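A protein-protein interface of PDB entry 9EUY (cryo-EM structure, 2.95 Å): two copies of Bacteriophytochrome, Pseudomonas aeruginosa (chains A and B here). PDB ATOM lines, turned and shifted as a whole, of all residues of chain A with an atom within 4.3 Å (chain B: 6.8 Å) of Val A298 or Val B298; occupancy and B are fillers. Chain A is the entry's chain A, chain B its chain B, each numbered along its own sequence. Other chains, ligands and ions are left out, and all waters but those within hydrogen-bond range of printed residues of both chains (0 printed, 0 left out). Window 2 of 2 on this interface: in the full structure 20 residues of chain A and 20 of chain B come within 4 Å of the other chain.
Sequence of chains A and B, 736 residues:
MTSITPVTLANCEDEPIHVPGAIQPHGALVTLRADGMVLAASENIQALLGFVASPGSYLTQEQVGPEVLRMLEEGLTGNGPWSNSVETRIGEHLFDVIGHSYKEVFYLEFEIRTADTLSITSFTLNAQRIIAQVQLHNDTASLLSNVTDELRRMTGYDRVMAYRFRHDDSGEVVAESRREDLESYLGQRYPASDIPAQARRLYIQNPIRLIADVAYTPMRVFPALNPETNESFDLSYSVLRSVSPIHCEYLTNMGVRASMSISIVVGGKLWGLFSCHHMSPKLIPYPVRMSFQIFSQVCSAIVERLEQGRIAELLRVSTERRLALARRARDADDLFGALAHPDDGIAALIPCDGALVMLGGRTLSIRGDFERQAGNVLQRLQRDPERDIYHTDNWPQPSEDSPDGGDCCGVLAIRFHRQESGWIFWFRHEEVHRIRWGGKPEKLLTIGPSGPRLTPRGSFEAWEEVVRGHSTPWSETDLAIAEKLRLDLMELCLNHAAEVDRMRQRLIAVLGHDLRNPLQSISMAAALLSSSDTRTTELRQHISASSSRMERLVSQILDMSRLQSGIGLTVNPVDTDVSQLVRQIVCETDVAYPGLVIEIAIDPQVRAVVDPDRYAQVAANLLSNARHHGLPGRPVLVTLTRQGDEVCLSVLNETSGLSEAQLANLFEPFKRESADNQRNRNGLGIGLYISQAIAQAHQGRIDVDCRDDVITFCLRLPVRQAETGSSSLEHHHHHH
The side-chain amide nitrogen (NE2) of Gln B135 sits at hydrogen-bond distance from the side-chain amide oxygen (OE1) of Gln A297 (2.4 Å).
The backbone carbonyl oxygen (O) of Ile B131 sits at hydrogen-bond distance from the side-chain amide nitrogen (NE2) of Gln B135 (3.2 Å).
Among the printed residues, pairs that only touch across the chains: Val A298 with Val B298 (3.8 Å), Ile A131 with Ile B294 (3.8 Å) and Ile A294 with Ile B131 (3.8 Å).
Of chain B, only Val B298 comes within 4 Å of Val A298.
Val B298 touches just one residue of chain A: Val A298 (3.8 Å).
Of the printed residues of chain A, Ile B294 touches Ile A131 (3.8 Å).
Of the printed residues of chain A, Gln B135 touches Gln A297.
The nearest printed residue of chain B that does not touch Ile A131 is Gln B297 (4.8 Å).
Hydrophobic or aromatic side chains of chain B that line the printed part of chain A: Ile B131, Ile B294 and Val B298.
Of the 10 printed residues of chain A, 4 touch a printed residue of chain B.
Printed residues of chain A that touch a printed residue of chain B: Ile A131, Ile A294, Gln A297 and Val A298.
Among the printed residues, 4 pairs touch across the chains.
Among the printed residues, no Asp or Glu carboxylate lies within 4 Å of a Lys or Arg side-chain nitrogen of the other chain.
Ile A131 touches Ile B294, and with the chains exchanged Ile A294 touches Ile B131.
Val A298 touches its own counterpart, Val B298.
Of the 4 pairs that touch across the chains among the printed residues, 3 have their exchanged pair printed and touching as well.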
ATOM      1  N   ILE A 131     -30.460   4.652  -8.040  1.00  0.00           N
ATOM      2  CA  ILE A 131     -29.337   5.531  -7.717  1.00  0.00           C
ATOM      3  C   ILE A 131     -28.786   6.179  -8.982  1.00  0.00           C
ATOM      4  O   ILE A 131     -28.436   7.365  -8.990  1.00  0.00           O
ATOM      5  CB  ILE A 131     -28.246   4.756  -6.956  1.00  0.00           C
ATOM      6  CG1 ILE A 131     -28.801   4.192  -5.652  1.00  0.00           C
ATOM      7  CG2 ILE A 131     -27.067   5.661  -6.657  1.00  0.00           C
ATOM      8  CD1 ILE A 131     -27.910   3.154  -5.013  1.00  0.00           C
ATOM      9  N   ILE A 294     -26.849   4.319   0.330  1.00  0.00           N
ATOM     10  CA  ILE A 294     -26.109   5.049  -0.692  1.00  0.00           C
ATOM     11  C   ILE A 294     -27.079   5.884  -1.509  1.00  0.00           C
ATOM     12  O   ILE A 294     -26.756   6.997  -1.940  1.00  0.00           O
ATOM     13  CB  ILE A 294     -25.299   4.085  -1.571  1.00  0.00           C
ATOM     14  CG1 ILE A 294     -24.192   3.446  -0.748  1.00  0.00           C
ATOM     15  CG2 ILE A 294     -24.693   4.817  -2.752  1.00  0.00           C
ATOM     16  CD1 ILE A 294     -23.650   2.232  -1.380  1.00  0.00           C
ATOM     17  N   PHE A 295     -28.272   5.346  -1.755  1.00  0.00           N
ATOM     18  CA  PHE A 295     -29.308   6.122  -2.420  1.00  0.00           C
ATOM     19  C   PHE A 295     -29.647   7.374  -1.626  1.00  0.00           C
ATOM     20  O   PHE A 295     -29.856   8.438  -2.204  1.00  0.00           O
ATOM     21  CB  PHE A 295     -30.565   5.279  -2.612  1.00  0.00           C
ATOM     22  CG  PHE A 295     -31.728   6.062  -3.128  1.00  0.00           C
ATOM     23  CD1 PHE A 295     -31.608   6.832  -4.270  1.00  0.00           C
ATOM     24  CD2 PHE A 295     -32.930   6.067  -2.446  1.00  0.00           C
ATOM     25  CE1 PHE A 295     -32.670   7.569  -4.732  1.00  0.00           C
ATOM     26  CE2 PHE A 295     -33.994   6.800  -2.906  1.00  0.00           C
ATOM     27  CZ  PHE A 295     -33.863   7.552  -4.050  1.00  0.00           C
ATOM     28  N   SER A 296     -29.761   7.250  -0.304  1.00  0.00           N
ATOM     29  CA  SER A 296     -30.009   8.407   0.547  1.00  0.00           C
ATOM     30  C   SER A 296     -28.912   9.451   0.407  1.00  0.00           C
ATOM     31  O   SER A 296     -29.198  10.645   0.285  1.00  0.00           O
ATOM     32  CB  SER A 296     -30.134   7.967   2.003  1.00  0.00           C
ATOM     33  OG  SER A 296     -30.124   9.083   2.877  1.00  0.00           O
ATOM     34  N   GLN A 297     -27.652   9.019   0.379  1.00  0.00           N
ATOM     35  CA  GLN A 297     -26.549   9.971   0.234  1.00  0.00           C
ATOM     36  C   GLN A 297     -26.559  10.658  -1.134  1.00  0.00           C
ATOM     37  O   GLN A 297     -26.445  11.891  -1.231  1.00  0.00           O
ATOM     38  CB  GLN A 297     -25.218   9.263   0.472  1.00  0.00           C
ATOM     39  CG  GLN A 297     -24.979   8.877   1.922  1.00  0.00           C
ATOM     40  CD  GLN A 297     -23.778   7.973   2.091  1.00  0.00           C
ATOM     41  OE1 GLN A 297     -23.273   7.406   1.123  1.00  0.00           O
ATOM     42  NE2 GLN A 297     -23.307   7.840   3.324  1.00  0.00           N
ATOM     43  N   VAL A 298     -26.766   9.880  -2.196  1.00  0.00           N
ATOM     44  CA  VAL A 298     -26.815  10.432  -3.548  1.00  0.00           C
ATOM     45  C   VAL A 298     -28.016  11.356  -3.713  1.00  0.00           C
ATOM     46  O   VAL A 298     -27.897  12.458  -4.261  1.00  0.00           O
ATOM     47  CB  VAL A 298     -26.828   9.290  -4.578  1.00  0.00           C
ATOM     48  CG1 VAL A 298     -27.144   9.815  -5.955  1.00  0.00           C
ATOM     49  CG2 VAL A 298     -25.491   8.575  -4.583  1.00  0.00           C
ATOM     50  N   CYS A 299     -29.192  10.907  -3.280  1.00  0.00           N
ATOM     51  CA  CYS A 299     -30.398  11.722  -3.356  1.00  0.00           C
ATOM     52  C   CYS A 299     -30.248  13.005  -2.555  1.00  0.00           C
ATOM     53  O   CYS A 299     -30.728  14.058  -2.975  1.00  0.00           O
ATOM     54  CB  CYS A 299     -31.604  10.922  -2.870  1.00  0.00           C
ATOM     55  SG  CYS A 299     -33.175  11.794  -3.010  1.00  0.00           S
ATOM     56  N   SER A 300     -29.628  12.933  -1.375  1.00  0.00           N
ATOM     57  CA  SER A 300     -29.399  14.140  -0.590  1.00  0.00           C
ATOM     58  C   SER A 300     -28.514  15.127  -1.338  1.00  0.00           C
ATOM     59  O   SER A 300     -28.808  16.327  -1.375  1.00  0.00           O
ATOM     60  CB  SER A 300     -28.765  13.771   0.749  1.00  0.00           C
ATOM     61  OG  SER A 300     -29.650  12.996   1.536  1.00  0.00           O
ATOM     62  N   ALA A 301     -27.454  14.636  -1.986  1.00  0.00           N
ATOM     63  CA  ALA A 301     -26.585  15.532  -2.748  1.00  0.00           C
ATOM     64  C   ALA A 301     -27.305  16.125  -3.958  1.00  0.00           C
ATOM     65  O   ALA A 301     -27.171  17.322  -4.249  1.00  0.00           O
ATOM     66  CB  ALA A 301     -25.326  14.790  -3.190  1.00  0.00           C
ATOM     67  N   ILE A 302     -28.127  15.319  -4.628  1.00  0.00           N
ATOM     68  CA  ILE A 302     -28.885  15.792  -5.784  1.00  0.00           C
ATOM     69  C   ILE A 302     -29.930  16.821  -5.370  1.00  0.00           C
ATOM     70  O   ILE A 302     -30.090  17.854  -6.026  1.00  0.00           O
ATOM     71  CB  ILE A 302     -29.524  14.609  -6.531  1.00  0.00           C
ATOM     72  CG1 ILE A 302     -28.444  13.762  -7.197  1.00  0.00           C
ATOM     73  CG2 ILE A 302     -30.504  15.105  -7.571  1.00  0.00           C
ATOM     74  CD1 ILE A 302     -28.915  12.396  -7.588  1.00  0.00           C
ATOM     75  N   ILE B 130     -16.876   1.062  -0.109  1.00  0.00           N
ATOM     76  CA  ILE B 130     -15.980   2.060  -0.692  1.00  0.00           C
ATOM     77  C   ILE B 130     -16.767   3.326  -0.987  1.00  0.00           C
ATOM     78  O   ILE B 130     -16.347   4.438  -0.653  1.00  0.00           O
ATOM     79  CB  ILE B 130     -15.288   1.545  -1.966  1.00  0.00           C
ATOM     80  CG1 ILE B 130     -14.306   0.426  -1.681  1.00  0.00           C
ATOM     81  CG2 ILE B 130     -14.555   2.676  -2.650  1.00  0.00           C
ATOM     82  CD1 ILE B 130     -13.376   0.212  -2.862  1.00  0.00           C
ATOM     83  N   ILE B 131     -17.940   3.162  -1.599  1.00  0.00           N
ATOM     84  CA  ILE B 131     -18.786   4.302  -1.948  1.00  0.00           C
ATOM     85  C   ILE B 131     -19.092   5.138  -0.712  1.00  0.00           C
ATOM     86  O   ILE B 131     -19.075   6.375  -0.756  1.00  0.00           O
ATOM     87  CB  ILE B 131     -20.077   3.823  -2.636  1.00  0.00           C
ATOM     88  CG1 ILE B 131     -19.750   2.936  -3.835  1.00  0.00           C
ATOM     89  CG2 ILE B 131     -20.907   5.010  -3.081  1.00  0.00           C
ATOM     90  CD1 ILE B 131     -20.956   2.250  -4.426  1.00  0.00           C
ATOM     91  N   ALA B 132     -19.370   4.476   0.410  1.00  0.00           N
ATOM     92  CA  ALA B 132     -19.658   5.174   1.660  1.00  0.00           C
ATOM     93  C   ALA B 132     -18.414   5.829   2.264  1.00  0.00           C
ATOM     94  O   ALA B 132     -18.427   7.022   2.587  1.00  0.00           O
ATOM     95  CB  ALA B 132     -20.288   4.206   2.661  1.00  0.00           C
ATOM     96  N   VAL B 134     -15.578   6.729   0.942  1.00  0.00           N
ATOM     97  CA  VAL B 134     -14.904   7.760   0.152  1.00  0.00           C
ATOM     98  C   VAL B 134     -15.418   9.163   0.467  1.00  0.00           C
ATOM     99  O   VAL B 134     -14.699  10.148   0.261  1.00  0.00           O
ATOM    100  CB  VAL B 134     -15.038   7.418  -1.350  1.00  0.00           C
ATOM    101  CG1 VAL B 134     -14.632   8.581  -2.234  1.00  0.00           C
ATOM    102  CG2 VAL B 134     -14.164   6.236  -1.678  1.00  0.00           C
ATOM    103  N   GLN B 135     -16.621   9.280   1.027  1.00  0.00           N
ATOM    104  CA  GLN B 135     -17.143  10.589   1.399  1.00  0.00           C
ATOM    105  C   GLN B 135     -16.443  11.192   2.610  1.00  0.00           C
ATOM    106  O   GLN B 135     -16.606  12.389   2.864  1.00  0.00           O
ATOM    107  CB  GLN B 135     -18.646  10.492   1.669  1.00  0.00           C
ATOM    108  CG  GLN B 135     -19.462  10.128   0.445  1.00  0.00           C
ATOM    109  CD  GLN B 135     -20.869   9.694   0.784  1.00  0.00           C
ATOM    110  OE1 GLN B 135     -21.620  10.428   1.424  1.00  0.00           O
ATOM    111  NE2 GLN B 135     -21.243   8.501   0.336  1.00  0.00           N
ATOM    112  N   GLN B 293     -19.747   1.363 -11.028  1.00  0.00           N
ATOM    113  CA  GLN B 293     -20.263   2.475 -11.824  1.00  0.00           C
ATOM    114  C   GLN B 293     -20.874   3.543 -10.923  1.00  0.00           C
ATOM    115  O   GLN B 293     -20.667   4.751 -11.127  1.00  0.00           O
ATOM    116  CB  GLN B 293     -21.289   1.952 -12.824  1.00  0.00           C
ATOM    117  CG  GLN B 293     -22.130   3.014 -13.483  1.00  0.00           C
ATOM    118  CD  GLN B 293     -22.978   2.454 -14.601  1.00  0.00           C
ATOM    119  OE1 GLN B 293     -22.827   1.296 -14.989  1.00  0.00           O
ATOM    120  NE2 GLN B 293     -23.884   3.270 -15.121  1.00  0.00           N
ATOM    121  N   ILE B 294     -21.549   3.108  -9.860  1.00  0.00           N
ATOM    122  CA  ILE B 294     -22.068   4.077  -8.902  1.00  0.00           C
ATOM    123  C   ILE B 294     -20.917   4.677  -8.111  1.00  0.00           C
ATOM    124  O   ILE B 294     -20.939   5.859  -7.753  1.00  0.00           O
ATOM    125  CB  ILE B 294     -23.118   3.432  -7.984  1.00  0.00           C
ATOM    126  CG1 ILE B 294     -24.355   3.068  -8.789  1.00  0.00           C
ATOM    127  CG2 ILE B 294     -23.503   4.374  -6.863  1.00  0.00           C
ATOM    128  CD1 ILE B 294     -25.260   2.166  -8.055  1.00  0.00           C
ATOM    129  N   PHE B 295     -19.900   3.867  -7.816  1.00  0.00           N
ATOM    130  CA  PHE B 295     -18.701   4.401  -7.184  1.00  0.00           C
ATOM    131  C   PHE B 295     -18.053   5.465  -8.056  1.00  0.00           C
ATOM    132  O   PHE B 295     -17.575   6.476  -7.549  1.00  0.00           O
ATOM    133  CB  PHE B 295     -17.692   3.295  -6.897  1.00  0.00           C
ATOM    134  CG  PHE B 295     -16.372   3.817  -6.423  1.00  0.00           C
ATOM    135  CD1 PHE B 295     -16.297   4.637  -5.312  1.00  0.00           C
ATOM    136  CD2 PHE B 295     -15.211   3.528  -7.115  1.00  0.00           C
ATOM    137  CE1 PHE B 295     -15.087   5.141  -4.893  1.00  0.00           C
ATOM    138  CE2 PHE B 295     -13.998   4.024  -6.695  1.00  0.00           C
ATOM    139  CZ  PHE B 295     -13.938   4.830  -5.581  1.00  0.00           C
ATOM    140  N   SER B 296     -17.977   5.223  -9.363  1.00  0.00           N
ATOM    141  CA  SER B 296     -17.442   6.216 -10.287  1.00  0.00           C
ATOM    142  C   SER B 296     -18.226   7.518 -10.216  1.00  0.00           C
ATOM    143  O   SER B 296     -17.641   8.599 -10.123  1.00  0.00           O
ATOM    144  CB  SER B 296     -17.453   5.661 -11.708  1.00  0.00           C
ATOM    145  OG  SER B 296     -17.202   6.681 -12.657  1.00  0.00           O
ATOM    146  N   GLN B 297     -19.558   7.432 -10.208  1.00  0.00           N
ATOM    147  CA  GLN B 297     -20.368   8.651 -10.144  1.00  0.00           C
ATOM    148  C   GLN B 297     -20.212   9.385  -8.809  1.00  0.00           C
ATOM    149  O   GLN B 297     -20.010  10.611  -8.780  1.00  0.00           O
ATOM    150  CB  GLN B 297     -21.834   8.309 -10.402  1.00  0.00           C
ATOM    151  CG  GLN B 297     -22.119   7.875 -11.832  1.00  0.00           C
ATOM    152  CD  GLN B 297     -23.470   7.206 -11.985  1.00  0.00           C
ATOM    153  OE1 GLN B 297     -24.094   6.811 -11.001  1.00  0.00           O
ATOM    154  NE2 GLN B 297     -23.928   7.076 -13.224  1.00  0.00           N
ATOM    155  N   VAL B 298     -20.188   8.639  -7.705  1.00  0.00           N
ATOM    156  CA  VAL B 298     -20.034   9.241  -6.384  1.00  0.00           C
ATOM    157  C   VAL B 298     -18.636   9.823  -6.211  1.00  0.00           C
ATOM    158  O   VAL B 298     -18.475  10.950  -5.732  1.00  0.00           O
ATOM    159  CB  VAL B 298     -20.356   8.201  -5.296  1.00  0.00           C
ATOM    160  CG1 VAL B 298     -19.911   8.688  -3.941  1.00  0.00           C
ATOM    161  CG2 VAL B 298     -21.841   7.898  -5.284  1.00  0.00           C
ATOM    162  N   CYS B 299     -17.608   9.044  -6.541  1.00  0.00           N
ATOM    163  CA  CYS B 299     -16.234   9.512  -6.439  1.00  0.00           C
ATOM    164  C   CYS B 299     -15.993  10.713  -7.341  1.00  0.00           C
ATOM    165  O   CYS B 299     -15.235  11.613  -6.981  1.00  0.00           O
ATOM    166  CB  CYS B 299     -15.267   8.382  -6.786  1.00  0.00           C
ATOM    167  SG  CYS B 299     -13.526   8.798  -6.567  1.00  0.00           S
ATOM    168  N   SER B 300     -16.596  10.733  -8.533  1.00  0.00           N
ATOM    169  CA  SER B 300     -16.491  11.909  -9.386  1.00  0.00           C
ATOM    170  C   SER B 300     -17.097  13.135  -8.718  1.00  0.00           C
ATOM    171  O   SER B 300     -16.505  14.220  -8.748  1.00  0.00           O
ATOM    172  CB  SER B 300     -17.173  11.642 -10.726  1.00  0.00           C
ATOM    173  OG  SER B 300     -16.514  10.607 -11.434  1.00  0.00           O
ATOM    174  N   ALA B 301     -18.241  12.971  -8.050  1.00  0.00           N
ATOM    175  CA  ALA B 301     -18.847  14.109  -7.357  1.00  0.00           C
ATOM    176  C   ALA B 301     -17.990  14.571  -6.179  1.00  0.00           C
ATOM    177  O   ALA B 301     -17.784  15.777  -5.978  1.00  0.00           O
ATOM    178  CB  ALA B 301     -20.252  13.748  -6.885  1.00  0.00           C
ATOM    179  N   ILE B 302     -17.434  13.620  -5.431  1.00  0.00           N
ATOM    180  CA  ILE B 302     -16.583  13.944  -4.289  1.00  0.00           C
ATOM    181  C   ILE B 302     -15.302  14.630  -4.745  1.00  0.00           C
ATOM    182  O   ILE B 302     -14.881  15.629  -4.157  1.00  0.00           O
ATOM    183  CB  ILE B 302     -16.282  12.686  -3.459  1.00  0.00           C
ATOM    184  CG1 ILE B 302     -17.555  12.179  -2.793  1.00  0.00           C
ATOM    185  CG2 ILE B 302     -15.226  12.978  -2.413  1.00  0.00           C
ATOM    186  CD1 ILE B 302     -17.471  10.746  -2.384  1.00  0.00           C
ATOM    187  N   VAL B 303     -14.627  14.065  -5.745  1.00  0.00           N
ATOM    188  CA  VAL B 303     -13.407  14.673  -6.260  1.00  0.00           C
ATOM    189  C   VAL B 303     -13.694  16.059  -6.822  1.00  0.00           C
ATOM    190  O   VAL B 303     -12.879  16.974  -6.678  1.00  0.00           O
ATOM    191  CB  VAL B 303     -12.755  13.753  -7.309  1.00  0.00           C
ATOM    192  CG1 VAL B 303     -11.650  14.480  -8.042  1.00  0.00           C
ATOM    193  CG2 VAL B 303     -12.202  12.512  -6.640  1.00  0.00           C
ATOM    194  N   GLU B 304     -14.848  16.243  -7.470  1.00  0.00           N
ATOM    195  CA  GLU B 304     -15.196  17.573  -7.960  1.00  0.00           C
ATOM    196  C   GLU B 304     -15.336  18.561  -6.808  1.00  0.00           C
ATOM    197  O   GLU B 304     -14.828  19.687  -6.876  1.00  0.00           O
ATOM    198  CB  GLU B 304     -16.485  17.511  -8.777  1.00  0.00           C
ATOM    199  CG  GLU B 304     -16.896  18.844  -9.370  1.00  0.00           C
ATOM    200  CD  GLU B 304     -17.821  18.694 -10.561  1.00  0.00           C
ATOM    201  OE1 GLU B 304     -18.989  18.302 -10.361  1.00  0.00           O
ATOM    202  OE2 GLU B 304     -17.384  18.975 -11.697  1.00  0.00           O
